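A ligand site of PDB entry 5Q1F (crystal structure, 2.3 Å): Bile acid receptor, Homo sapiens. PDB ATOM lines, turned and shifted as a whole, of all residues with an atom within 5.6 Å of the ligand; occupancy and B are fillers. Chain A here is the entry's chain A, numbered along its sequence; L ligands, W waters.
The backbone carbonyl oxygen of Met 89 lies within hydrogen-bond range of the side-chain hydroxyl of Ser 93 (3.1 Å). O of Tyr 130 is in hydrogen-bond range of ND2 of Asn 98, at 2.8 Å. The side-chain sulfur of Met 51 lies within hydrogen-bond range of the guanidinium group of Arg 25, 3.2 Å away. SD of Met 126 lies within hydrogen-bond range of OH of Tyr 130 (3.6 Å). The backbone carbonyl oxygen (O) of Ile 34 lies within hydrogen-bond range of the guanidinium group (NE) of Arg 112, 3.5 Å away. O of Ser 116 lies close to ND2 of Asn 44 (3.3 Å). The side-chain amide oxygen (OE1) of Gln 24 sits at hydrogen-bond distance from the guanidinium group (NH1) of Arg 92, 3.3 Å away. The backbone carbonyl oxygen of Ile 113 sits at hydrogen-bond distance from the side-chain hydroxyl of Ser 116.
N of Phe 97 sits close to F1 of the ligand, 3.0 Å away. CB of Arg 25 touches O4 of the ligand (3.95 Å). Ile 30 touches the ligand. CD1 of Ile 34 touches C19 of the ligand (3.7 Å). Asn 44 touches the ligand (OD1 to C22, 3.6 Å). Ile 47 touches the ligand (CG2 to C21, 3.8 Å). Leu 48 touches the ligand (CD1 to N2, 3.8 Å). CB of Met 51 touches O3 of the ligand, at 3.4 Å. CD2 of His 55 touches O5 of the ligand, 3.3 Å away. CE of Met 89 touches C28 of the ligand, at 3.5 Å. CE1 of Phe 90 touches N2 of the ligand, at 3.6 Å. Ile 96 touches the ligand. Ile 113 touches the ligand (CD1 to C17, 3.6 Å). Ser 116 touches the ligand. Ile 118 touches the ligand (CD1 to O1, 3.8 Å). Met 126 touches the ligand. Met 211 touches the ligand. CD2 of Leu 212 touches C14 of the ligand (3.9 Å). Trp 215 touches the ligand. Trp 230 touches the ligand (CH2 to C14, 3.9 Å). Hydrophobic or aromatic side chains that line the ligand: Ile 30, Ile 34, Ile 47, Leu 48, Met 51, His 55, Met 89, Phe 90, Ile 96, Phe 97, Ile 113, Ile 118, Met 126, Tyr 130, Met 211, Leu 212, Trp 215 and Trp 230. Within 4 Å of the ligand: Arg 25, Ile 30, Ile 34, Asn 44, Ile 47, Leu 48, Met 51, His 55, Met 89, Phe 90, Arg 92, Ser 93, Ile 96, Phe 97, Ile 113, Ser 116, Ile 118, Met 126, Tyr 130, Met 211, Leu 212, Trp 215 and Trp 230. The nearest printed residue that does not touch the ligand is Leu 109 (4.03 Å).
Water W2 lies within hydrogen-bond range of an oxygen (O5) of the ligand (2.7 Å), the side-chain amide oxygen of Asn 54 (2.7 Å) and the backbone carbonyl oxygen of Met 51 (2.8 Å). Water W1 lies within hydrogen-bond range of O5 of the ligand (2.7 Å) and NE2 of Gln 24 (3.4 Å).
The guanidinium group (NE) of Arg 92 is in salt-bridge range of an oxygen (O4) of the ligand (3.1 Å). OG of Ser 93 is in hydrogen-bond range of O2 of the ligand (3.0 Å). N1 of the ligand lies within hydrogen-bond range of OH of Tyr 130.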
ATOM      1  N   GLN A  24       7.104  30.049   4.739  1.00  0.00           N
ATOM      2  CA  GLN A  24       7.195  29.437   6.064  1.00  0.00           C
ATOM      3  C   GLN A  24       6.858  30.421   7.201  1.00  0.00           C
ATOM      4  O   GLN A  24       6.763  31.639   6.966  1.00  0.00           O
ATOM      5  CB  GLN A  24       8.592  28.850   6.285  1.00  0.00           C
ATOM      6  CG  GLN A  24       8.747  27.451   5.736  1.00  0.00           C
ATOM      7  CD  GLN A  24      10.100  26.863   6.003  1.00  0.00           C
ATOM      8  OE1 GLN A  24      11.138  27.484   5.774  1.00  0.00           O
ATOM      9  NE2 GLN A  24      10.114  25.621   6.462  1.00  0.00           N
ATOM     10  N   ARG A  25       6.708  29.884   8.424  1.00  0.00           N
ATOM     11  CA  ARG A  25       6.396  30.657   9.639  1.00  0.00           C
ATOM     12  C   ARG A  25       7.613  31.502  10.037  1.00  0.00           C
ATOM     13  O   ARG A  25       8.746  31.036   9.922  1.00  0.00           O
ATOM     14  CB  ARG A  25       6.015  29.679  10.771  1.00  0.00           C
ATOM     15  CG  ARG A  25       5.138  30.286  11.851  1.00  0.00           C
ATOM     16  CD  ARG A  25       4.443  29.202  12.640  1.00  0.00           C
ATOM     17  NE  ARG A  25       3.056  29.006  12.215  1.00  0.00           N
ATOM     18  CZ  ARG A  25       2.232  28.086  12.698  1.00  0.00           C
ATOM     19  NH1 ARG A  25       2.647  27.246  13.637  1.00  0.00           N
ATOM     20  NH2 ARG A  25       0.990  27.988  12.247  1.00  0.00           N
ATOM     21  N   ILE A  30       8.038  32.417  16.411  1.00  0.00           N
ATOM     22  CA  ILE A  30       8.242  31.144  17.126  1.00  0.00           C
ATOM     23  C   ILE A  30       9.086  31.332  18.398  1.00  0.00           C
ATOM     24  O   ILE A  30       8.684  30.845  19.468  1.00  0.00           O
ATOM     25  CB  ILE A  30       8.838  30.085  16.133  1.00  0.00           C
ATOM     26  CG1 ILE A  30       7.851  29.768  14.993  1.00  0.00           C
ATOM     27  CG2 ILE A  30       9.272  28.793  16.854  1.00  0.00           C
ATOM     28  CD1 ILE A  30       8.479  29.673  13.649  1.00  0.00           C
ATOM     29  N   THR A  31      10.254  32.015  18.291  1.00  0.00           N
ATOM     30  CA  THR A  31      11.166  32.246  19.426  1.00  0.00           C
ATOM     31  C   THR A  31      10.594  33.215  20.447  1.00  0.00           C
ATOM     32  O   THR A  31      10.850  33.032  21.625  1.00  0.00           O
ATOM     33  CB  THR A  31      12.566  32.665  18.983  1.00  0.00           C
ATOM     34  OG1 THR A  31      12.488  33.796  18.105  1.00  0.00           O
ATOM     35  CG2 THR A  31      13.324  31.537  18.345  1.00  0.00           C
ATOM     36  N   ILE A  34       8.248  31.143  22.789  1.00  0.00           N
ATOM     37  CA  ILE A  34       9.064  30.315  23.677  1.00  0.00           C
ATOM     38  C   ILE A  34       9.710  31.177  24.787  1.00  0.00           C
ATOM     39  O   ILE A  34       9.686  30.775  25.954  1.00  0.00           O
ATOM     40  CB  ILE A  34      10.112  29.475  22.871  1.00  0.00           C
ATOM     41  CG1 ILE A  34       9.426  28.499  21.884  1.00  0.00           C
ATOM     42  CG2 ILE A  34      11.106  28.719  23.794  1.00  0.00           C
ATOM     43  CD1 ILE A  34      10.324  28.007  20.707  1.00  0.00           C
ATOM     44  N   ASN A  44       3.651  22.589  25.891  1.00  0.00           N
ATOM     45  CA  ASN A  44       4.743  22.442  24.922  1.00  0.00           C
ATOM     46  C   ASN A  44       4.517  21.289  23.979  1.00  0.00           C
ATOM     47  O   ASN A  44       4.859  21.410  22.794  1.00  0.00           O
ATOM     48  CB  ASN A  44       6.086  22.333  25.637  1.00  0.00           C
ATOM     49  CG  ASN A  44       6.607  23.655  26.137  1.00  0.00           C
ATOM     50  OD1 ASN A  44       6.428  24.712  25.517  1.00  0.00           O
ATOM     51  ND2 ASN A  44       7.265  23.638  27.280  1.00  0.00           N
ATOM     52  N   ILE A  47       1.926  22.576  21.589  1.00  0.00           N
ATOM     53  CA  ILE A  47       2.587  23.550  20.703  1.00  0.00           C
ATOM     54  C   ILE A  47       3.367  22.767  19.625  1.00  0.00           C
ATOM     55  O   ILE A  47       3.217  23.060  18.440  1.00  0.00           O
ATOM     56  CB  ILE A  47       3.504  24.550  21.496  1.00  0.00           C
ATOM     57  CG1 ILE A  47       2.673  25.537  22.360  1.00  0.00           C
ATOM     58  CG2 ILE A  47       4.449  25.331  20.558  1.00  0.00           C
ATOM     59  CD1 ILE A  47       3.453  26.122  23.591  1.00  0.00           C
ATOM     60  N   LEU A  48       4.131  21.743  20.033  1.00  0.00           N
ATOM     61  CA  LEU A  48       4.927  20.908  19.132  1.00  0.00           C
ATOM     62  C   LEU A  48       4.076  20.220  18.049  1.00  0.00           C
ATOM     63  O   LEU A  48       4.444  20.311  16.882  1.00  0.00           O
ATOM     64  CB  LEU A  48       5.796  19.892  19.914  1.00  0.00           C
ATOM     65  CG  LEU A  48       6.573  18.833  19.066  1.00  0.00           C
ATOM     66  CD1 LEU A  48       7.643  19.464  18.177  1.00  0.00           C
ATOM     67  CD2 LEU A  48       7.192  17.808  19.944  1.00  0.00           C
ATOM     68  N   MET A  51       2.760  22.897  15.560  1.00  0.00           N
ATOM     69  CA  MET A  51       3.890  23.389  14.759  1.00  0.00           C
ATOM     70  C   MET A  51       4.288  22.337  13.735  1.00  0.00           C
ATOM     71  O   MET A  51       4.582  22.688  12.590  1.00  0.00           O
ATOM     72  CB  MET A  51       5.108  23.725  15.655  1.00  0.00           C
ATOM     73  CG  MET A  51       4.920  24.940  16.517  1.00  0.00           C
ATOM     74  SD  MET A  51       5.037  26.463  15.593  1.00  0.00           S
ATOM     75  CE  MET A  51       4.682  27.643  16.909  1.00  0.00           C
ATOM     76  N   ASN A  54       1.464  22.006  10.903  1.00  0.00           N
ATOM     77  CA  ASN A  54       1.608  23.147   9.986  1.00  0.00           C
ATOM     78  C   ASN A  54       2.837  22.982   9.086  1.00  0.00           C
ATOM     79  O   ASN A  54       2.737  23.202   7.890  1.00  0.00           O
ATOM     80  CB  ASN A  54       1.621  24.480  10.738  1.00  0.00           C
ATOM     81  CG  ASN A  54       2.014  25.669   9.880  1.00  0.00           C
ATOM     82  OD1 ASN A  54       3.158  26.121   9.904  1.00  0.00           O
ATOM     83  ND2 ASN A  54       1.094  26.160   9.056  1.00  0.00           N
ATOM     84  N   HIS A  55       3.987  22.559   9.659  1.00  0.00           N
ATOM     85  CA  HIS A  55       5.245  22.324   8.953  1.00  0.00           C
ATOM     86  C   HIS A  55       5.083  21.313   7.815  1.00  0.00           C
ATOM     87  O   HIS A  55       5.642  21.545   6.743  1.00  0.00           O
ATOM     88  CB  HIS A  55       6.407  21.905   9.911  1.00  0.00           C
ATOM     89  CG  HIS A  55       7.725  21.841   9.204  1.00  0.00           C
ATOM     90  ND1 HIS A  55       8.141  20.681   8.552  1.00  0.00           N
ATOM     91  CD2 HIS A  55       8.620  22.820   8.945  1.00  0.00           C
ATOM     92  CE1 HIS A  55       9.270  20.987   7.932  1.00  0.00           C
ATOM     93  NE2 HIS A  55       9.620  22.266   8.155  1.00  0.00           N
ATOM     94  N   MET A  89      11.951  19.134   9.264  1.00  0.00           N
ATOM     95  CA  MET A  89      11.476  19.842  10.439  1.00  0.00           C
ATOM     96  C   MET A  89      12.610  20.133  11.424  1.00  0.00           C
ATOM     97  O   MET A  89      12.660  21.234  11.958  1.00  0.00           O
ATOM     98  CB  MET A  89      10.308  19.124  11.110  1.00  0.00           C
ATOM     99  CG  MET A  89       9.471  20.099  11.896  1.00  0.00           C
ATOM    100  SD  MET A  89       8.499  19.310  13.171  1.00  0.00           S
ATOM    101  CE  MET A  89       8.029  20.722  14.098  1.00  0.00           C
ATOM    102  N   PHE A  90      13.552  19.168  11.624  1.00  0.00           N
ATOM    103  CA  PHE A  90      14.732  19.370  12.483  1.00  0.00           C
ATOM    104  C   PHE A  90      15.706  20.395  11.896  1.00  0.00           C
ATOM    105  O   PHE A  90      16.288  21.191  12.633  1.00  0.00           O
ATOM    106  CB  PHE A  90      15.458  18.051  12.841  1.00  0.00           C
ATOM    107  CG  PHE A  90      14.782  17.318  13.982  1.00  0.00           C
ATOM    108  CD1 PHE A  90      14.912  17.776  15.300  1.00  0.00           C
ATOM    109  CD2 PHE A  90      14.001  16.198  13.744  1.00  0.00           C
ATOM    110  CE1 PHE A  90      14.247  17.138  16.344  1.00  0.00           C
ATOM    111  CE2 PHE A  90      13.351  15.552  14.803  1.00  0.00           C
ATOM    112  CZ  PHE A  90      13.465  16.024  16.089  1.00  0.00           C
ATOM    113  N   ARG A  92      14.816  22.905   9.971  1.00  0.00           N
ATOM    114  CA  ARG A  92      14.141  24.182  10.176  1.00  0.00           C
ATOM    115  C   ARG A  92      14.256  24.671  11.652  1.00  0.00           C
ATOM    116  O   ARG A  92      14.389  25.866  11.882  1.00  0.00           O
ATOM    117  CB  ARG A  92      12.679  24.118   9.668  1.00  0.00           C
ATOM    118  CG  ARG A  92      11.857  25.399   9.855  1.00  0.00           C
ATOM    119  CD  ARG A  92      12.337  26.580   9.012  1.00  0.00           C
ATOM    120  NE  ARG A  92      11.612  27.815   9.329  1.00  0.00           N
ATOM    121  CZ  ARG A  92      11.916  29.009   8.823  1.00  0.00           C
ATOM    122  NH1 ARG A  92      12.916  29.144   7.970  1.00  0.00           N
ATOM    123  NH2 ARG A  92      11.205  30.068   9.157  1.00  0.00           N
ATOM    124  N   SER A  93      14.268  23.746  12.618  1.00  0.00           N
ATOM    125  CA  SER A  93      14.426  24.068  14.051  1.00  0.00           C
ATOM    126  C   SER A  93      15.846  24.546  14.344  1.00  0.00           C
ATOM    127  O   SER A  93      16.035  25.411  15.196  1.00  0.00           O
ATOM    128  CB  SER A  93      14.128  22.843  14.902  1.00  0.00           C
ATOM    129  OG  SER A  93      12.775  22.463  14.748  1.00  0.00           O
ATOM    130  N   ALA A  94      16.838  23.967  13.638  1.00  0.00           N
ATOM    131  CA  ALA A  94      18.244  24.308  13.755  1.00  0.00           C
ATOM    132  C   ALA A  94      18.452  25.723  13.204  1.00  0.00           C
ATOM    133  O   ALA A  94      19.180  26.509  13.803  1.00  0.00           O
ATOM    134  CB  ALA A  94      19.099  23.303  12.981  1.00  0.00           C
ATOM    135  N   ILE A  96      16.122  28.223  13.011  1.00  0.00           N
ATOM    136  CA  ILE A  96      15.491  29.112  13.985  1.00  0.00           C
ATOM    137  C   ILE A  96      16.369  29.224  15.234  1.00  0.00           C
ATOM    138  O   ILE A  96      16.586  30.336  15.704  1.00  0.00           O
ATOM    139  CB  ILE A  96      14.038  28.659  14.298  1.00  0.00           C
ATOM    140  CG1 ILE A  96      13.142  28.750  13.015  1.00  0.00           C
ATOM    141  CG2 ILE A  96      13.440  29.455  15.464  1.00  0.00           C
ATOM    142  CD1 ILE A  96      11.851  28.011  13.095  1.00  0.00           C
ATOM    143  N   PHE A  97      16.939  28.105  15.723  1.00  0.00           N
ATOM    144  CA  PHE A  97      17.810  28.078  16.894  1.00  0.00           C
ATOM    145  C   PHE A  97      19.053  28.996  16.758  1.00  0.00           C
ATOM    146  O   PHE A  97      19.450  29.620  17.744  1.00  0.00           O
ATOM    147  CB  PHE A  97      18.260  26.635  17.207  1.00  0.00           C
ATOM    148  CG  PHE A  97      19.061  26.468  18.477  1.00  0.00           C
ATOM    149  CD1 PHE A  97      18.428  26.381  19.709  1.00  0.00           C
ATOM    150  CD2 PHE A  97      20.449  26.419  18.455  1.00  0.00           C
ATOM    151  CE1 PHE A  97      19.166  26.249  20.891  1.00  0.00           C
ATOM    152  CE2 PHE A  97      21.193  26.284  19.630  1.00  0.00           C
ATOM    153  CZ  PHE A  97      20.549  26.192  20.843  1.00  0.00           C
ATOM    154  N   ASN A  98      19.643  29.066  15.554  1.00  0.00           N
ATOM    155  CA  ASN A  98      20.864  29.800  15.295  1.00  0.00           C
ATOM    156  C   ASN A  98      20.664  31.226  14.767  1.00  0.00           C
ATOM    157  O   ASN A  98      21.654  31.877  14.412  1.00  0.00           O
ATOM    158  CB  ASN A  98      21.772  28.989  14.387  1.00  0.00           C
ATOM    159  CG  ASN A  98      22.287  27.764  15.089  1.00  0.00           C
ATOM    160  OD1 ASN A  98      23.073  27.838  16.038  1.00  0.00           O
ATOM    161  ND2 ASN A  98      21.827  26.604  14.657  1.00  0.00           N
ATOM    162  N   LEU A 109      16.546  30.548  25.400  1.00  0.00           N
ATOM    163  CA  LEU A 109      15.891  29.727  24.385  1.00  0.00           C
ATOM    164  C   LEU A 109      16.310  28.264  24.552  1.00  0.00           C
ATOM    165  O   LEU A 109      15.450  27.389  24.520  1.00  0.00           O
ATOM    166  CB  LEU A 109      16.200  30.246  22.972  1.00  0.00           C
ATOM    167  CG  LEU A 109      15.569  29.493  21.776  1.00  0.00           C
ATOM    168  CD1 LEU A 109      14.060  29.725  21.686  1.00  0.00           C
ATOM    169  CD2 LEU A 109      16.227  29.892  20.472  1.00  0.00           C
ATOM    170  N   ARG A 112      14.779  26.790  27.844  1.00  0.00           N
ATOM    171  CA  ARG A 112      13.345  26.555  27.649  1.00  0.00           C
ATOM    172  C   ARG A 112      13.099  25.283  26.820  1.00  0.00           C
ATOM    173  O   ARG A 112      12.205  24.502  27.142  1.00  0.00           O
ATOM    174  CB  ARG A 112      12.657  27.764  27.024  1.00  0.00           C
ATOM    175  CG  ARG A 112      12.525  28.960  27.948  1.00  0.00           C
ATOM    176  CD  ARG A 112      11.209  29.039  28.703  1.00  0.00           C
ATOM    177  NE  ARG A 112      10.945  30.399  29.149  1.00  0.00           N
ATOM    178  CZ  ARG A 112      11.332  30.903  30.321  1.00  0.00           C
ATOM    179  NH1 ARG A 112      12.031  30.176  31.173  1.00  0.00           N
ATOM    180  NH2 ARG A 112      11.038  32.161  30.630  1.00  0.00           N
ATOM    181  N   ILE A 113      13.927  25.046  25.786  1.00  0.00           N
ATOM    182  CA  ILE A 113      13.853  23.852  24.945  1.00  0.00           C
ATOM    183  C   ILE A 113      14.303  22.618  25.759  1.00  0.00           C
ATOM    184  O   ILE A 113      13.694  21.563  25.633  1.00  0.00           O
ATOM    185  CB  ILE A 113      14.579  24.040  23.570  1.00  0.00           C
ATOM    186  CG1 ILE A 113      13.889  25.155  22.746  1.00  0.00           C
ATOM    187  CG2 ILE A 113      14.592  22.747  22.756  1.00  0.00           C
ATOM    188  CD1 ILE A 113      14.696  25.745  21.643  1.00  0.00           C
ATOM    189  N   SER A 116      11.375  21.646  28.017  1.00  0.00           N
ATOM    190  CA  SER A 116      10.108  21.589  27.282  1.00  0.00           C
ATOM    191  C   SER A 116       9.252  20.354  27.585  1.00  0.00           C
ATOM    192  O   SER A 116       8.035  20.419  27.464  1.00  0.00           O
ATOM    193  CB  SER A 116      10.341  21.720  25.778  1.00  0.00           C
ATOM    194  OG  SER A 116      11.150  20.672  25.250  1.00  0.00           O
ATOM    195  N   ILE A 118      10.743  17.082  26.568  1.00  0.00           N
ATOM    196  CA  ILE A 118      11.537  16.102  25.843  1.00  0.00           C
ATOM    197  C   ILE A 118      12.425  15.308  26.835  1.00  0.00           C
ATOM    198  O   ILE A 118      12.899  15.864  27.841  1.00  0.00           O
ATOM    199  CB  ILE A 118      12.363  16.809  24.718  1.00  0.00           C
ATOM    200  CG1 ILE A 118      13.203  15.816  23.876  1.00  0.00           C
ATOM    201  CG2 ILE A 118      13.232  17.954  25.247  1.00  0.00           C
ATOM    202  CD1 ILE A 118      12.496  15.278  22.692  1.00  0.00           C
ATOM    203  N   MET A 126      20.393  16.423  20.056  1.00  0.00           N
ATOM    204  CA  MET A 126      19.656  17.515  19.443  1.00  0.00           C
ATOM    205  C   MET A 126      20.441  18.829  19.460  1.00  0.00           C
ATOM    206  O   MET A 126      20.541  19.472  18.419  1.00  0.00           O
ATOM    207  CB  MET A 126      18.273  17.681  20.073  1.00  0.00           C
ATOM    208  CG  MET A 126      17.317  18.519  19.262  1.00  0.00           C
ATOM    209  SD  MET A 126      15.701  18.749  20.061  1.00  0.00           S
ATOM    210  CE  MET A 126      16.169  19.661  21.490  1.00  0.00           C
ATOM    211  N   TYR A 130      22.206  21.096  16.405  1.00  0.00           N
ATOM    212  CA  TYR A 130      21.892  22.534  16.337  1.00  0.00           C
ATOM    213  C   TYR A 130      23.152  23.403  16.390  1.00  0.00           C
ATOM    214  O   TYR A 130      23.265  24.348  15.611  1.00  0.00           O
ATOM    215  CB  TYR A 130      20.937  22.940  17.482  1.00  0.00           C
ATOM    216  CG  TYR A 130      19.517  22.413  17.405  1.00  0.00           C
ATOM    217  CD1 TYR A 130      19.058  21.704  16.291  1.00  0.00           C
ATOM    218  CD2 TYR A 130      18.602  22.642  18.444  1.00  0.00           C
ATOM    219  CE1 TYR A 130      17.761  21.206  16.227  1.00  0.00           C
ATOM    220  CE2 TYR A 130      17.295  22.166  18.376  1.00  0.00           C
ATOM    221  CZ  TYR A 130      16.885  21.450  17.262  1.00  0.00           C
ATOM    222  OH  TYR A 130      15.608  20.947  17.188  1.00  0.00           O
ATOM    223  N   HIS A 208      12.631   9.362  16.119  1.00  0.00           N
ATOM    224  CA  HIS A 208      11.630  10.449  16.113  1.00  0.00           C
ATOM    225  C   HIS A 208      10.298  10.072  16.822  1.00  0.00           C
ATOM    226  O   HIS A 208       9.740  10.892  17.577  1.00  0.00           O
ATOM    227  CB  HIS A 208      11.381  10.978  14.692  1.00  0.00           C
ATOM    228  CG  HIS A 208      10.703  10.014  13.745  1.00  0.00           C
ATOM    229  ND1 HIS A 208      11.439   9.182  12.930  1.00  0.00           N
ATOM    230  CD2 HIS A 208       9.386   9.822  13.501  1.00  0.00           C
ATOM    231  CE1 HIS A 208      10.553   8.482  12.231  1.00  0.00           C
ATOM    232  NE2 HIS A 208       9.298   8.844  12.534  1.00  0.00           N
ATOM    233  N   MET A 211      10.867  10.071  20.506  1.00  0.00           N
ATOM    234  CA  MET A 211      11.004  11.465  20.969  1.00  0.00           C
ATOM    235  C   MET A 211       9.654  12.069  21.326  1.00  0.00           C
ATOM    236  O   MET A 211       9.583  12.899  22.224  1.00  0.00           O
ATOM    237  CB  MET A 211      11.686  12.329  19.909  1.00  0.00           C
ATOM    238  CG  MET A 211      13.177  12.223  19.921  1.00  0.00           C
ATOM    239  SD  MET A 211      13.925  13.227  18.629  1.00  0.00           S
ATOM    240  CE  MET A 211      14.200  14.729  19.529  1.00  0.00           C
ATOM    241  N   LEU A 212       8.604  11.664  20.620  1.00  0.00           N
ATOM    242  CA  LEU A 212       7.244  12.124  20.884  1.00  0.00           C
ATOM    243  C   LEU A 212       6.579  11.297  21.968  1.00  0.00           C
ATOM    244  O   LEU A 212       5.881  11.869  22.814  1.00  0.00           O
ATOM    245  CB  LEU A 212       6.398  12.085  19.615  1.00  0.00           C
ATOM    246  CG  LEU A 212       6.851  12.925  18.448  1.00  0.00           C
ATOM    247  CD1 LEU A 212       5.991  12.635  17.246  1.00  0.00           C
ATOM    248  CD2 LEU A 212       6.745  14.381  18.762  1.00  0.00           C
ATOM    249  N   TRP A 215       7.871  11.965  25.642  1.00  0.00           N
ATOM    250  CA  TRP A 215       7.626  13.315  26.133  1.00  0.00           C
ATOM    251  C   TRP A 215       6.935  13.205  27.502  1.00  0.00           C
ATOM    252  O   TRP A 215       6.070  12.340  27.670  1.00  0.00           O
ATOM    253  CB  TRP A 215       6.750  14.097  25.142  1.00  0.00           C
ATOM    254  CG  TRP A 215       6.784  15.586  25.321  1.00  0.00           C
ATOM    255  CD1 TRP A 215       6.047  16.313  26.205  1.00  0.00           C
ATOM    256  CD2 TRP A 215       7.574  16.521  24.572  1.00  0.00           C
ATOM    257  NE1 TRP A 215       6.334  17.654  26.057  1.00  0.00           N
ATOM    258  CE2 TRP A 215       7.260  17.807  25.064  1.00  0.00           C
ATOM    259  CE3 TRP A 215       8.532  16.397  23.547  1.00  0.00           C
ATOM    260  CZ2 TRP A 215       7.869  18.967  24.546  1.00  0.00           C
ATOM    261  CZ3 TRP A 215       9.126  17.549  23.035  1.00  0.00           C
ATOM    262  CH2 TRP A 215       8.794  18.810  23.537  1.00  0.00           C
ATOM    263  N   TRP A 230       4.892  11.032  11.147  1.00  0.00           N
ATOM    264  CA  TRP A 230       5.707  10.540  12.261  1.00  0.00           C
ATOM    265  C   TRP A 230       5.120   9.161  12.493  1.00  0.00           C
ATOM    266  O   TRP A 230       3.936   8.983  12.249  1.00  0.00           O
ATOM    267  CB  TRP A 230       5.537  11.454  13.483  1.00  0.00           C
ATOM    268  CG  TRP A 230       6.085  12.855  13.304  1.00  0.00           C
ATOM    269  CD1 TRP A 230       5.556  13.832  12.512  1.00  0.00           C
ATOM    270  CD2 TRP A 230       7.252  13.415  13.913  1.00  0.00           C
ATOM    271  NE1 TRP A 230       6.327  14.971  12.605  1.00  0.00           N
ATOM    272  CE2 TRP A 230       7.352  14.753  13.473  1.00  0.00           C
ATOM    273  CE3 TRP A 230       8.236  12.914  14.803  1.00  0.00           C
ATOM    274  CZ2 TRP A 230       8.382  15.606  13.912  1.00  0.00           C
ATOM    275  CZ3 TRP A 230       9.213  13.780  15.263  1.00  0.00           C
ATOM    276  CH2 TRP A 230       9.299  15.101  14.793  1.00  0.00           C
HETATM  277  N1  LIG L   1      13.604  22.554  18.505  1.00  0.00           N
HETATM  278  C1  LIG L   1      12.027  20.690  18.880  1.00  0.00           C
HETATM  279  C2  LIG L   1      13.480  23.932  18.328  1.00  0.00           C
HETATM  280  C3  LIG L   1       9.143  23.471  17.486  1.00  0.00           C
HETATM  281  C4  LIG L   1      12.154  24.326  18.396  1.00  0.00           C
HETATM  282  C5  LIG L   1      11.645  19.842  17.828  1.00  0.00           C
HETATM  283  C6  LIG L   1       9.949  22.960  18.772  1.00  0.00           C
HETATM  284  C7  LIG L   1      12.070  20.134  20.161  1.00  0.00           C
HETATM  285  C8  LIG L   1      11.378  18.044  19.226  1.00  0.00           C
HETATM  286  C9  LIG L   1       9.436  23.583  20.098  1.00  0.00           C
HETATM  287  C10 LIG L   1      14.062  26.206  17.982  1.00  0.00           C
HETATM  288  C11 LIG L   1       9.332  23.954  12.537  1.00  0.00           C
HETATM  289  C12 LIG L   1      11.744  18.790  20.348  1.00  0.00           C
HETATM  290  C13 LIG L   1       9.246  24.040  15.066  1.00  0.00           C
HETATM  291  C14 LIG L   1      10.241  16.058  18.497  1.00  0.00           C
HETATM  292  O1  LIG L   1      11.061  16.721  19.450  1.00  0.00           O
HETATM  293  O2  LIG L   1      11.601  20.393  16.601  1.00  0.00           O
HETATM  294  C15 LIG L   1      11.256  19.545  15.497  1.00  0.00           C
HETATM  295  N2  LIG L   1      11.324  18.550  17.984  1.00  0.00           N
HETATM  296  C16 LIG L   1      12.365  22.120  18.667  1.00  0.00           C
HETATM  297  C17 LIG L   1      14.468  24.903  18.114  1.00  0.00           C
HETATM  298  F1  LIG L   1      15.009  27.153  17.775  1.00  0.00           F
HETATM  299  C18 LIG L   1      12.736  26.609  18.047  1.00  0.00           C
HETATM  300  C19 LIG L   1      11.757  25.655  18.248  1.00  0.00           C
HETATM  301  N3  LIG L   1      11.431  23.138  18.607  1.00  0.00           N
HETATM  302  C20 LIG L   1       8.129  22.935  20.559  1.00  0.00           C
HETATM  303  C21 LIG L   1       7.601  23.581  21.852  1.00  0.00           C
HETATM  304  C22 LIG L   1       8.631  23.507  22.976  1.00  0.00           C
HETATM  305  C23 LIG L   1       9.990  24.102  22.536  1.00  0.00           C
HETATM  306  C24 LIG L   1      10.481  23.465  21.225  1.00  0.00           C
HETATM  307  O3  LIG L   1       7.945  23.732  17.560  1.00  0.00           O
HETATM  308  N4  LIG L   1       9.837  23.587  16.339  1.00  0.00           N
HETATM  309  C25 LIG L   1       9.102  25.558  15.024  1.00  0.00           C
HETATM  310  C26 LIG L   1       8.388  26.023  13.734  1.00  0.00           C
HETATM  311  C27 LIG L   1       9.124  25.512  12.460  1.00  0.00           C
HETATM  312  C28 LIG L   1      10.027  23.556  13.864  1.00  0.00           C
HETATM  313  C29 LIG L   1       8.404  25.930  11.184  1.00  0.00           C
HETATM  314  O4  LIG L   1       8.906  26.990  10.604  1.00  0.00           O
HETATM  315  O5  LIG L   1       7.444  25.325  10.757  1.00  0.00           O
HETATM  316  O   HOH W   1       7.183  26.114   8.202  1.00  0.00           O
HETATM  317  O   HOH W   2       4.970  25.324  11.796  1.00  0.00           O
